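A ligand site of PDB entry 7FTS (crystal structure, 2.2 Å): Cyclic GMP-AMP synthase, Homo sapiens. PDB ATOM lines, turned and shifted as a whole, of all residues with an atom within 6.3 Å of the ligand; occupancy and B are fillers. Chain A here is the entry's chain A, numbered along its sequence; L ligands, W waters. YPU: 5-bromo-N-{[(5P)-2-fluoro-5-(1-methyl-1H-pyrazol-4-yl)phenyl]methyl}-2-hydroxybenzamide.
ND2 of Asn 322 lies within hydrogen-bond range of O20 of the ligand (2.6 Å).
N of Phe 219 sits at hydrogen-bond distance from O1 of the ligand.
The backbone carbonyl oxygen (O) of Leu 217 lies close to a nitrogen (N5) of the ligand (3.3 Å).
The side-chain amide nitrogen of Asn 322 lies within hydrogen-bond range of the side-chain hydroxyl of Tyr 276 (3.4 Å).
The backbone NH (N) of Asn 322 is in hydrogen-bond range of the backbone carbonyl oxygen (O) of Phe 328 (2.8 Å).
OD1 of Asn 322 is in hydrogen-bond range of N of Ile 325 (2.8 Å).
The side-chain amide oxygen of Asn 322 lies within hydrogen-bond range of the backbone NH of Phe 324 (2.6 Å).
The side-chain carboxylate (OE2) of Glu 223 lies within salt-bridge range of the side-chain amino group (NZ) of Lys 279 (3.2 Å).
N of Tyr 276 lies close to OG of Ser 274, 3.5 Å away.
The side-chain hydroxyl (OG1) of Thr 280 sits at hydrogen-bond distance from the backbone carbonyl oxygen (O) of Tyr 276, 2.7 Å away.
N of Ser 274 lies within hydrogen-bond range of ND1 of His 277.
Residues that only touch the ligand: Arg 216, Ala 87, Glu 223, Tyr 276, Phe 328, Phe 283, Ser 220, Ile 325, Ser 218, Phe 324, Lys 279, Tyr 88 and Ser 274.
Hydrophobic or aromatic side chains that line the ligand: Ala 87, Phe 219, Tyr 276, Phe 283, Phe 324, Ile 325 and Phe 328.
Of the 22 residues printed, 16 come within 4 Å of the ligand.
Water W1 lies within hydrogen-bond range of the side-chain hydroxyl of Thr 280 (2.7 Å), the backbone NH of Tyr 323 (2.8 Å), an oxygen (O20) of the ligand (3.0 Å) and the side-chain amide nitrogen of Asn 322 (3.5 Å).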
ATOM      1  N   ALA A  87     -15.419 -23.624 -10.140  1.00  0.00           N
ATOM      2  CA  ALA A  87     -14.126 -23.364  -9.523  1.00  0.00           C
ATOM      3  C   ALA A  87     -13.247 -22.336 -10.245  1.00  0.00           C
ATOM      4  O   ALA A  87     -12.188 -22.000  -9.722  1.00  0.00           O
ATOM      5  CB  ALA A  87     -13.327 -24.668  -9.403  1.00  0.00           C
ATOM      6  N   TYR A  88     -13.643 -21.834 -11.410  1.00  0.00           N
ATOM      7  CA  TYR A  88     -12.856 -20.814 -12.077  1.00  0.00           C
ATOM      8  C   TYR A  88     -13.656 -19.522 -12.159  1.00  0.00           C
ATOM      9  O   TYR A  88     -14.862 -19.551 -12.437  1.00  0.00           O
ATOM     10  CB  TYR A  88     -12.389 -21.303 -13.463  1.00  0.00           C
ATOM     11  CG  TYR A  88     -11.447 -22.511 -13.379  1.00  0.00           C
ATOM     12  CD1 TYR A  88     -10.101 -22.353 -13.076  1.00  0.00           C
ATOM     13  CD2 TYR A  88     -11.919 -23.797 -13.603  1.00  0.00           C
ATOM     14  CE1 TYR A  88      -9.251 -23.456 -12.994  1.00  0.00           C
ATOM     15  CE2 TYR A  88     -11.085 -24.900 -13.531  1.00  0.00           C
ATOM     16  CZ  TYR A  88      -9.743 -24.729 -13.222  1.00  0.00           C
ATOM     17  OH  TYR A  88      -8.900 -25.822 -13.147  1.00  0.00           O
ATOM     18  N   LYS A 202      -5.174 -19.639 -13.874  1.00  0.00           N
ATOM     19  CA  LYS A 202      -5.620 -20.989 -14.196  1.00  0.00           C
ATOM     20  C   LYS A 202      -4.533 -21.878 -14.829  1.00  0.00           C
ATOM     21  O   LYS A 202      -4.346 -23.034 -14.403  1.00  0.00           O
ATOM     22  CB  LYS A 202      -6.876 -20.919 -15.091  1.00  0.00           C
ATOM     23  CG  LYS A 202      -6.790 -21.498 -16.529  1.00  0.00           C
ATOM     24  CD  LYS A 202      -7.542 -22.827 -16.756  1.00  0.00           C
ATOM     25  CE  LYS A 202      -7.248 -23.407 -18.151  1.00  0.00           C
ATOM     26  NZ  LYS A 202      -7.182 -24.916 -18.183  1.00  0.00           N
ATOM     27  N   ARG A 216      -8.498 -19.482  -9.958  1.00  0.00           N
ATOM     28  CA  ARG A 216      -8.955 -20.616  -9.162  1.00  0.00           C
ATOM     29  C   ARG A 216      -8.570 -20.369  -7.712  1.00  0.00           C
ATOM     30  O   ARG A 216      -7.689 -19.571  -7.421  1.00  0.00           O
ATOM     31  CB  ARG A 216      -8.323 -21.942  -9.624  1.00  0.00           C
ATOM     32  CG  ARG A 216      -6.903 -22.056  -9.087  1.00  0.00           C
ATOM     33  CD  ARG A 216      -6.384 -23.434  -9.276  1.00  0.00           C
ATOM     34  NE  ARG A 216      -4.945 -23.556  -9.016  1.00  0.00           N
ATOM     35  CZ  ARG A 216      -4.418 -23.782  -7.825  1.00  0.00           C
ATOM     36  NH1 ARG A 216      -5.185 -23.901  -6.752  1.00  0.00           N
ATOM     37  NH2 ARG A 216      -3.106 -23.886  -7.722  1.00  0.00           N
ATOM     38  N   LEU A 217      -9.218 -21.115  -6.807  1.00  0.00           N
ATOM     39  CA  LEU A 217      -8.979 -20.963  -5.371  1.00  0.00           C
ATOM     40  C   LEU A 217      -7.763 -21.773  -4.905  1.00  0.00           C
ATOM     41  O   LEU A 217      -7.500 -22.877  -5.393  1.00  0.00           O
ATOM     42  CB  LEU A 217     -10.225 -21.428  -4.616  1.00  0.00           C
ATOM     43  CG  LEU A 217     -11.416 -20.485  -4.608  1.00  0.00           C
ATOM     44  CD1 LEU A 217     -12.701 -21.186  -4.135  1.00  0.00           C
ATOM     45  CD2 LEU A 217     -11.051 -19.380  -3.672  1.00  0.00           C
ATOM     46  N   SER A 218      -7.035 -21.226  -3.922  1.00  0.00           N
ATOM     47  CA  SER A 218      -5.853 -21.898  -3.360  1.00  0.00           C
ATOM     48  C   SER A 218      -6.043 -22.138  -1.870  1.00  0.00           C
ATOM     49  O   SER A 218      -6.167 -21.173  -1.099  1.00  0.00           O
ATOM     50  CB  SER A 218      -4.578 -21.079  -3.606  1.00  0.00           C
ATOM     51  OG  SER A 218      -3.502 -21.496  -2.772  1.00  0.00           O
ATOM     52  N   PHE A 219      -6.056 -23.412  -1.450  1.00  0.00           N
ATOM     53  CA  PHE A 219      -6.327 -23.718  -0.040  1.00  0.00           C
ATOM     54  C   PHE A 219      -5.149 -24.372   0.661  1.00  0.00           C
ATOM     55  O   PHE A 219      -5.330 -25.085   1.651  1.00  0.00           O
ATOM     56  CB  PHE A 219      -7.573 -24.588   0.082  1.00  0.00           C
ATOM     57  CG  PHE A 219      -8.869 -23.838  -0.125  1.00  0.00           C
ATOM     58  CD1 PHE A 219      -9.336 -22.988   0.854  1.00  0.00           C
ATOM     59  CD2 PHE A 219      -9.606 -24.005  -1.272  1.00  0.00           C
ATOM     60  CE1 PHE A 219     -10.520 -22.300   0.673  1.00  0.00           C
ATOM     61  CE2 PHE A 219     -10.812 -23.346  -1.458  1.00  0.00           C
ATOM     62  CZ  PHE A 219     -11.256 -22.472  -0.496  1.00  0.00           C
ATOM     63  N   SER A 220      -3.931 -24.115   0.190  1.00  0.00           N
ATOM     64  CA  SER A 220      -2.738 -24.684   0.814  1.00  0.00           C
ATOM     65  C   SER A 220      -2.631 -24.281   2.278  1.00  0.00           C
ATOM     66  O   SER A 220      -2.137 -25.049   3.109  1.00  0.00           O
ATOM     67  CB  SER A 220      -1.494 -24.243   0.040  1.00  0.00           C
ATOM     68  OG  SER A 220      -1.608 -24.645  -1.319  1.00  0.00           O
ATOM     69  N   HIS A 221      -3.069 -23.070   2.614  1.00  0.00           N
ATOM     70  CA  HIS A 221      -2.971 -22.630   4.000  1.00  0.00           C
ATOM     71  C   HIS A 221      -3.875 -23.444   4.899  1.00  0.00           C
ATOM     72  O   HIS A 221      -3.598 -23.593   6.095  1.00  0.00           O
ATOM     73  CB  HIS A 221      -3.312 -21.131   4.095  1.00  0.00           C
ATOM     74  CG  HIS A 221      -4.695 -20.790   3.637  1.00  0.00           C
ATOM     75  ND1 HIS A 221      -5.189 -21.182   2.415  1.00  0.00           N
ATOM     76  CD2 HIS A 221      -5.668 -20.052   4.215  1.00  0.00           C
ATOM     77  CE1 HIS A 221      -6.421 -20.717   2.269  1.00  0.00           C
ATOM     78  NE2 HIS A 221      -6.742 -20.032   3.350  1.00  0.00           N
ATOM     79  N   GLU A 223      -5.039 -26.773   4.220  1.00  0.00           N
ATOM     80  CA  GLU A 223      -4.286 -28.020   4.283  1.00  0.00           C
ATOM     81  C   GLU A 223      -3.241 -27.981   5.367  1.00  0.00           C
ATOM     82  O   GLU A 223      -3.170 -28.872   6.213  1.00  0.00           O
ATOM     83  CB  GLU A 223      -3.597 -28.284   2.945  1.00  0.00           C
ATOM     84  CG  GLU A 223      -2.561 -29.367   3.051  1.00  0.00           C
ATOM     85  CD  GLU A 223      -1.748 -29.480   1.783  1.00  0.00           C
ATOM     86  OE1 GLU A 223      -0.909 -30.409   1.698  1.00  0.00           O
ATOM     87  OE2 GLU A 223      -1.942 -28.658   0.868  1.00  0.00           O
ATOM     88  N   SER A 274      -0.931 -34.229 -10.254  1.00  0.00           N
ATOM     89  CA  SER A 274      -0.084 -33.520  -9.306  1.00  0.00           C
ATOM     90  C   SER A 274      -0.394 -33.972  -7.877  1.00  0.00           C
ATOM     91  O   SER A 274      -1.333 -34.735  -7.620  1.00  0.00           O
ATOM     92  CB  SER A 274      -0.259 -32.008  -9.439  1.00  0.00           C
ATOM     93  OG  SER A 274      -1.585 -31.645  -9.080  1.00  0.00           O
ATOM     94  N   TYR A 276      -1.740 -32.319  -5.676  1.00  0.00           N
ATOM     95  CA  TYR A 276      -3.111 -31.896  -5.412  1.00  0.00           C
ATOM     96  C   TYR A 276      -4.106 -33.049  -5.549  1.00  0.00           C
ATOM     97  O   TYR A 276      -5.051 -33.168  -4.755  1.00  0.00           O
ATOM     98  CB  TYR A 276      -3.421 -30.745  -6.359  1.00  0.00           C
ATOM     99  CG  TYR A 276      -4.832 -30.494  -6.773  1.00  0.00           C
ATOM    100  CD1 TYR A 276      -5.761 -30.034  -5.858  1.00  0.00           C
ATOM    101  CD2 TYR A 276      -5.210 -30.614  -8.098  1.00  0.00           C
ATOM    102  CE1 TYR A 276      -7.067 -29.753  -6.251  1.00  0.00           C
ATOM    103  CE2 TYR A 276      -6.507 -30.347  -8.506  1.00  0.00           C
ATOM    104  CZ  TYR A 276      -7.431 -29.917  -7.580  1.00  0.00           C
ATOM    105  OH  TYR A 276      -8.722 -29.628  -7.978  1.00  0.00           O
ATOM    106  N   HIS A 277      -3.934 -33.923  -6.546  1.00  0.00           N
ATOM    107  CA  HIS A 277      -4.905 -35.011  -6.700  1.00  0.00           C
ATOM    108  C   HIS A 277      -4.743 -36.036  -5.589  1.00  0.00           C
ATOM    109  O   HIS A 277      -5.706 -36.695  -5.196  1.00  0.00           O
ATOM    110  CB  HIS A 277      -4.752 -35.659  -8.077  1.00  0.00           C
ATOM    111  CG  HIS A 277      -5.044 -34.727  -9.229  1.00  0.00           C
ATOM    112  ND1 HIS A 277      -4.046 -34.190 -10.002  1.00  0.00           N
ATOM    113  CD2 HIS A 277      -6.211 -34.235  -9.707  1.00  0.00           C
ATOM    114  CE1 HIS A 277      -4.583 -33.415 -10.934  1.00  0.00           C
ATOM    115  NE2 HIS A 277      -5.892 -33.412 -10.764  1.00  0.00           N
ATOM    116  N   LYS A 279      -3.359 -35.282  -2.346  1.00  0.00           N
ATOM    117  CA  LYS A 279      -3.867 -34.647  -1.137  1.00  0.00           C
ATOM    118  C   LYS A 279      -5.364 -34.774  -1.082  1.00  0.00           C
ATOM    119  O   LYS A 279      -5.925 -35.245  -0.082  1.00  0.00           O
ATOM    120  CB  LYS A 279      -3.467 -33.172  -1.097  1.00  0.00           C
ATOM    121  CG  LYS A 279      -1.980 -32.962  -1.206  1.00  0.00           C
ATOM    122  CD  LYS A 279      -1.665 -31.468  -1.237  1.00  0.00           C
ATOM    123  CE  LYS A 279      -0.178 -31.223  -1.271  1.00  0.00           C
ATOM    124  NZ  LYS A 279       0.071 -29.752  -1.311  1.00  0.00           N
ATOM    125  N   THR A 280      -6.045 -34.382  -2.174  1.00  0.00           N
ATOM    126  CA  THR A 280      -7.500 -34.404  -2.184  1.00  0.00           C
ATOM    127  C   THR A 280      -8.009 -35.769  -1.802  1.00  0.00           C
ATOM    128  O   THR A 280      -8.749 -35.911  -0.827  1.00  0.00           O
ATOM    129  CB  THR A 280      -8.046 -34.018  -3.566  1.00  0.00           C
ATOM    130  OG1 THR A 280      -7.561 -32.718  -3.932  1.00  0.00           O
ATOM    131  CG2 THR A 280      -9.556 -33.960  -3.525  1.00  0.00           C
ATOM    132  N   PHE A 283      -7.486 -36.630   1.967  1.00  0.00           N
ATOM    133  CA  PHE A 283      -8.402 -36.048   2.940  1.00  0.00           C
ATOM    134  C   PHE A 283      -9.767 -36.693   2.863  1.00  0.00           C
ATOM    135  O   PHE A 283     -10.465 -36.780   3.885  1.00  0.00           O
ATOM    136  CB  PHE A 283      -8.492 -34.529   2.748  1.00  0.00           C
ATOM    137  CG  PHE A 283      -7.281 -33.777   3.244  1.00  0.00           C
ATOM    138  CD1 PHE A 283      -6.772 -34.019   4.501  1.00  0.00           C
ATOM    139  CD2 PHE A 283      -6.642 -32.853   2.452  1.00  0.00           C
ATOM    140  CE1 PHE A 283      -5.657 -33.343   4.960  1.00  0.00           C
ATOM    141  CE2 PHE A 283      -5.528 -32.187   2.913  1.00  0.00           C
ATOM    142  CZ  PHE A 283      -5.031 -32.431   4.151  1.00  0.00           C
ATOM    143  N   ASN A 322     -13.433 -32.293  -5.655  1.00  0.00           N
ATOM    144  CA  ASN A 322     -12.575 -31.339  -4.964  1.00  0.00           C
ATOM    145  C   ASN A 322     -12.964 -31.358  -3.492  1.00  0.00           C
ATOM    146  O   ASN A 322     -14.125 -31.557  -3.148  1.00  0.00           O
ATOM    147  CB  ASN A 322     -12.767 -29.945  -5.546  1.00  0.00           C
ATOM    148  CG  ASN A 322     -11.906 -28.904  -4.877  1.00  0.00           C
ATOM    149  OD1 ASN A 322     -12.265 -28.361  -3.815  1.00  0.00           O
ATOM    150  ND2 ASN A 322     -10.774 -28.580  -5.493  1.00  0.00           N
ATOM    151  N   TYR A 323     -11.974 -31.210  -2.619  1.00  0.00           N
ATOM    152  CA  TYR A 323     -12.269 -31.368  -1.205  1.00  0.00           C
ATOM    153  C   TYR A 323     -13.050 -30.173  -0.678  1.00  0.00           C
ATOM    154  O   TYR A 323     -13.731 -30.287   0.375  1.00  0.00           O
ATOM    155  CB  TYR A 323     -10.962 -31.559  -0.414  1.00  0.00           C
ATOM    156  CG  TYR A 323     -11.209 -32.101   0.970  1.00  0.00           C
ATOM    157  CD1 TYR A 323     -11.775 -33.334   1.145  1.00  0.00           C
ATOM    158  CD2 TYR A 323     -10.913 -31.359   2.102  1.00  0.00           C
ATOM    159  CE1 TYR A 323     -12.028 -33.838   2.406  1.00  0.00           C
ATOM    160  CE2 TYR A 323     -11.157 -31.863   3.368  1.00  0.00           C
ATOM    161  CZ  TYR A 323     -11.714 -33.084   3.509  1.00  0.00           C
ATOM    162  OH  TYR A 323     -11.962 -33.614   4.744  1.00  0.00           O
ATOM    163  N   PHE A 324     -12.961 -29.038  -1.375  1.00  0.00           N
ATOM    164  CA  PHE A 324     -13.545 -27.786  -0.935  1.00  0.00           C
ATOM    165  C   PHE A 324     -14.756 -27.416  -1.743  1.00  0.00           C
ATOM    166  O   PHE A 324     -15.616 -26.663  -1.270  1.00  0.00           O
ATOM    167  CB  PHE A 324     -12.510 -26.655  -1.033  1.00  0.00           C
ATOM    168  CG  PHE A 324     -11.359 -26.834  -0.087  1.00  0.00           C
ATOM    169  CD1 PHE A 324     -10.325 -27.721  -0.389  1.00  0.00           C
ATOM    170  CD2 PHE A 324     -11.311 -26.149   1.101  1.00  0.00           C
ATOM    171  CE1 PHE A 324      -9.302 -27.949   0.479  1.00  0.00           C
ATOM    172  CE2 PHE A 324     -10.261 -26.358   1.982  1.00  0.00           C
ATOM    173  CZ  PHE A 324      -9.263 -27.264   1.662  1.00  0.00           C
ATOM    174  N   ILE A 325     -14.861 -27.952  -2.949  1.00  0.00           N
ATOM    175  CA  ILE A 325     -15.905 -27.592  -3.893  1.00  0.00           C
ATOM    176  C   ILE A 325     -16.523 -28.886  -4.410  1.00  0.00           C
ATOM    177  O   ILE A 325     -16.128 -29.392  -5.473  1.00  0.00           O
ATOM    178  CB  ILE A 325     -15.319 -26.741  -5.036  1.00  0.00           C
ATOM    179  CG1 ILE A 325     -14.444 -25.611  -4.481  1.00  0.00           C
ATOM    180  CG2 ILE A 325     -16.435 -26.187  -5.935  1.00  0.00           C
ATOM    181  CD1 ILE A 325     -13.861 -24.741  -5.582  1.00  0.00           C
ATOM    182  N   PHE A 328     -17.007 -29.980  -8.197  1.00  0.00           N
ATOM    183  CA  PHE A 328     -15.900 -29.956  -9.141  1.00  0.00           C
ATOM    184  C   PHE A 328     -15.172 -31.300  -9.114  1.00  0.00           C
ATOM    185  O   PHE A 328     -14.583 -31.671  -8.085  1.00  0.00           O
ATOM    186  CB  PHE A 328     -14.971 -28.795  -8.805  1.00  0.00           C
ATOM    187  CG  PHE A 328     -13.850 -28.628  -9.746  1.00  0.00           C
ATOM    188  CD1 PHE A 328     -14.082 -28.494 -11.090  1.00  0.00           C
ATOM    189  CD2 PHE A 328     -12.559 -28.594  -9.283  1.00  0.00           C
ATOM    190  CE1 PHE A 328     -13.045 -28.352 -11.955  1.00  0.00           C
ATOM    191  CE2 PHE A 328     -11.514 -28.435 -10.160  1.00  0.00           C
ATOM    192  CZ  PHE A 328     -11.762 -28.318 -11.497  1.00  0.00           C
ATOM    193  N   LEU A 330     -12.247 -33.546 -10.179  1.00  0.00           N
ATOM    194  CA  LEU A 330     -10.875 -33.476 -10.657  1.00  0.00           C
ATOM    195  C   LEU A 330     -10.557 -34.491 -11.742  1.00  0.00           C
ATOM    196  O   LEU A 330      -9.580 -34.296 -12.489  1.00  0.00           O
ATOM    197  CB  LEU A 330      -9.880 -33.697  -9.517  1.00  0.00           C
ATOM    198  CG  LEU A 330     -10.122 -32.977  -8.204  1.00  0.00           C
ATOM    199  CD1 LEU A 330      -8.835 -32.900  -7.430  1.00  0.00           C
ATOM    200  CD2 LEU A 330     -10.722 -31.620  -8.434  1.00  0.00           C
HETATM  201  C10 YPU L   1      -8.114 -26.327  -9.414  1.00  0.00           C
HETATM  202  C11 YPU L   1      -7.091 -26.502  -8.488  1.00  0.00           C
HETATM  203  C13 YPU L   1      -5.725 -26.911  -8.893  1.00  0.00           C
HETATM  204  C17 YPU L   1      -5.243 -27.198 -10.184  1.00  0.00           C
HETATM  205  C18 YPU L   1      -2.261 -27.796  -8.443  1.00  0.00           C
HETATM  206  C21 YPU L   1      -6.849 -28.673  -2.056  1.00  0.00           C
HETATM  207  C22 YPU L   1      -5.831 -28.971  -1.182  1.00  0.00           C
HETATM  208  C24 YPU L   1      -4.756 -28.132  -1.013  1.00  0.00           C
HETATM  209  C25 YPU L   1      -4.701 -26.956  -1.731  1.00  0.00           C
HETATM  210  C12 YPU L   1      -7.368 -26.262  -7.131  1.00  0.00           C
HETATM  211  C14 YPU L   1      -4.648 -27.105  -8.074  1.00  0.00           C
HETATM  212  C2  YPU L   1      -5.703 -26.623  -2.629  1.00  0.00           C
HETATM  213  C3  YPU L   1      -6.796 -27.489  -2.789  1.00  0.00           C
HETATM  214  C4  YPU L   1      -7.908 -27.172  -3.739  1.00  0.00           C
HETATM  215  C6  YPU L   1      -8.922 -25.615  -5.264  1.00  0.00           C
HETATM  216  C7  YPU L   1      -8.625 -25.876  -6.712  1.00  0.00           C
HETATM  217  C8  YPU L   1      -9.608 -25.715  -7.682  1.00  0.00           C
HETATM  218  C9  YPU L   1      -9.372 -25.933  -9.011  1.00  0.00           C
HETATM  219  F19 YPU L   1     -10.831 -25.327  -7.280  1.00  0.00           F
HETATM  220  N15 YPU L   1      -3.604 -27.475  -8.870  1.00  0.00           N
HETATM  221  N16 YPU L   1      -3.969 -27.538 -10.156  1.00  0.00           N
HETATM  222  N5  YPU L   1      -7.827 -26.030  -4.405  1.00  0.00           N
HETATM  223  O1  YPU L   1      -5.626 -25.452  -3.307  1.00  0.00           O
HETATM  224  O20 YPU L   1      -8.855 -27.942  -3.884  1.00  0.00           O
HETATM  225 BR23 YPU L   1      -5.936 -30.565  -0.169  1.00  0.00          BR
HETATM  226  O   HOH W   1      -9.309 -30.821  -3.309  1.00  0.00           O
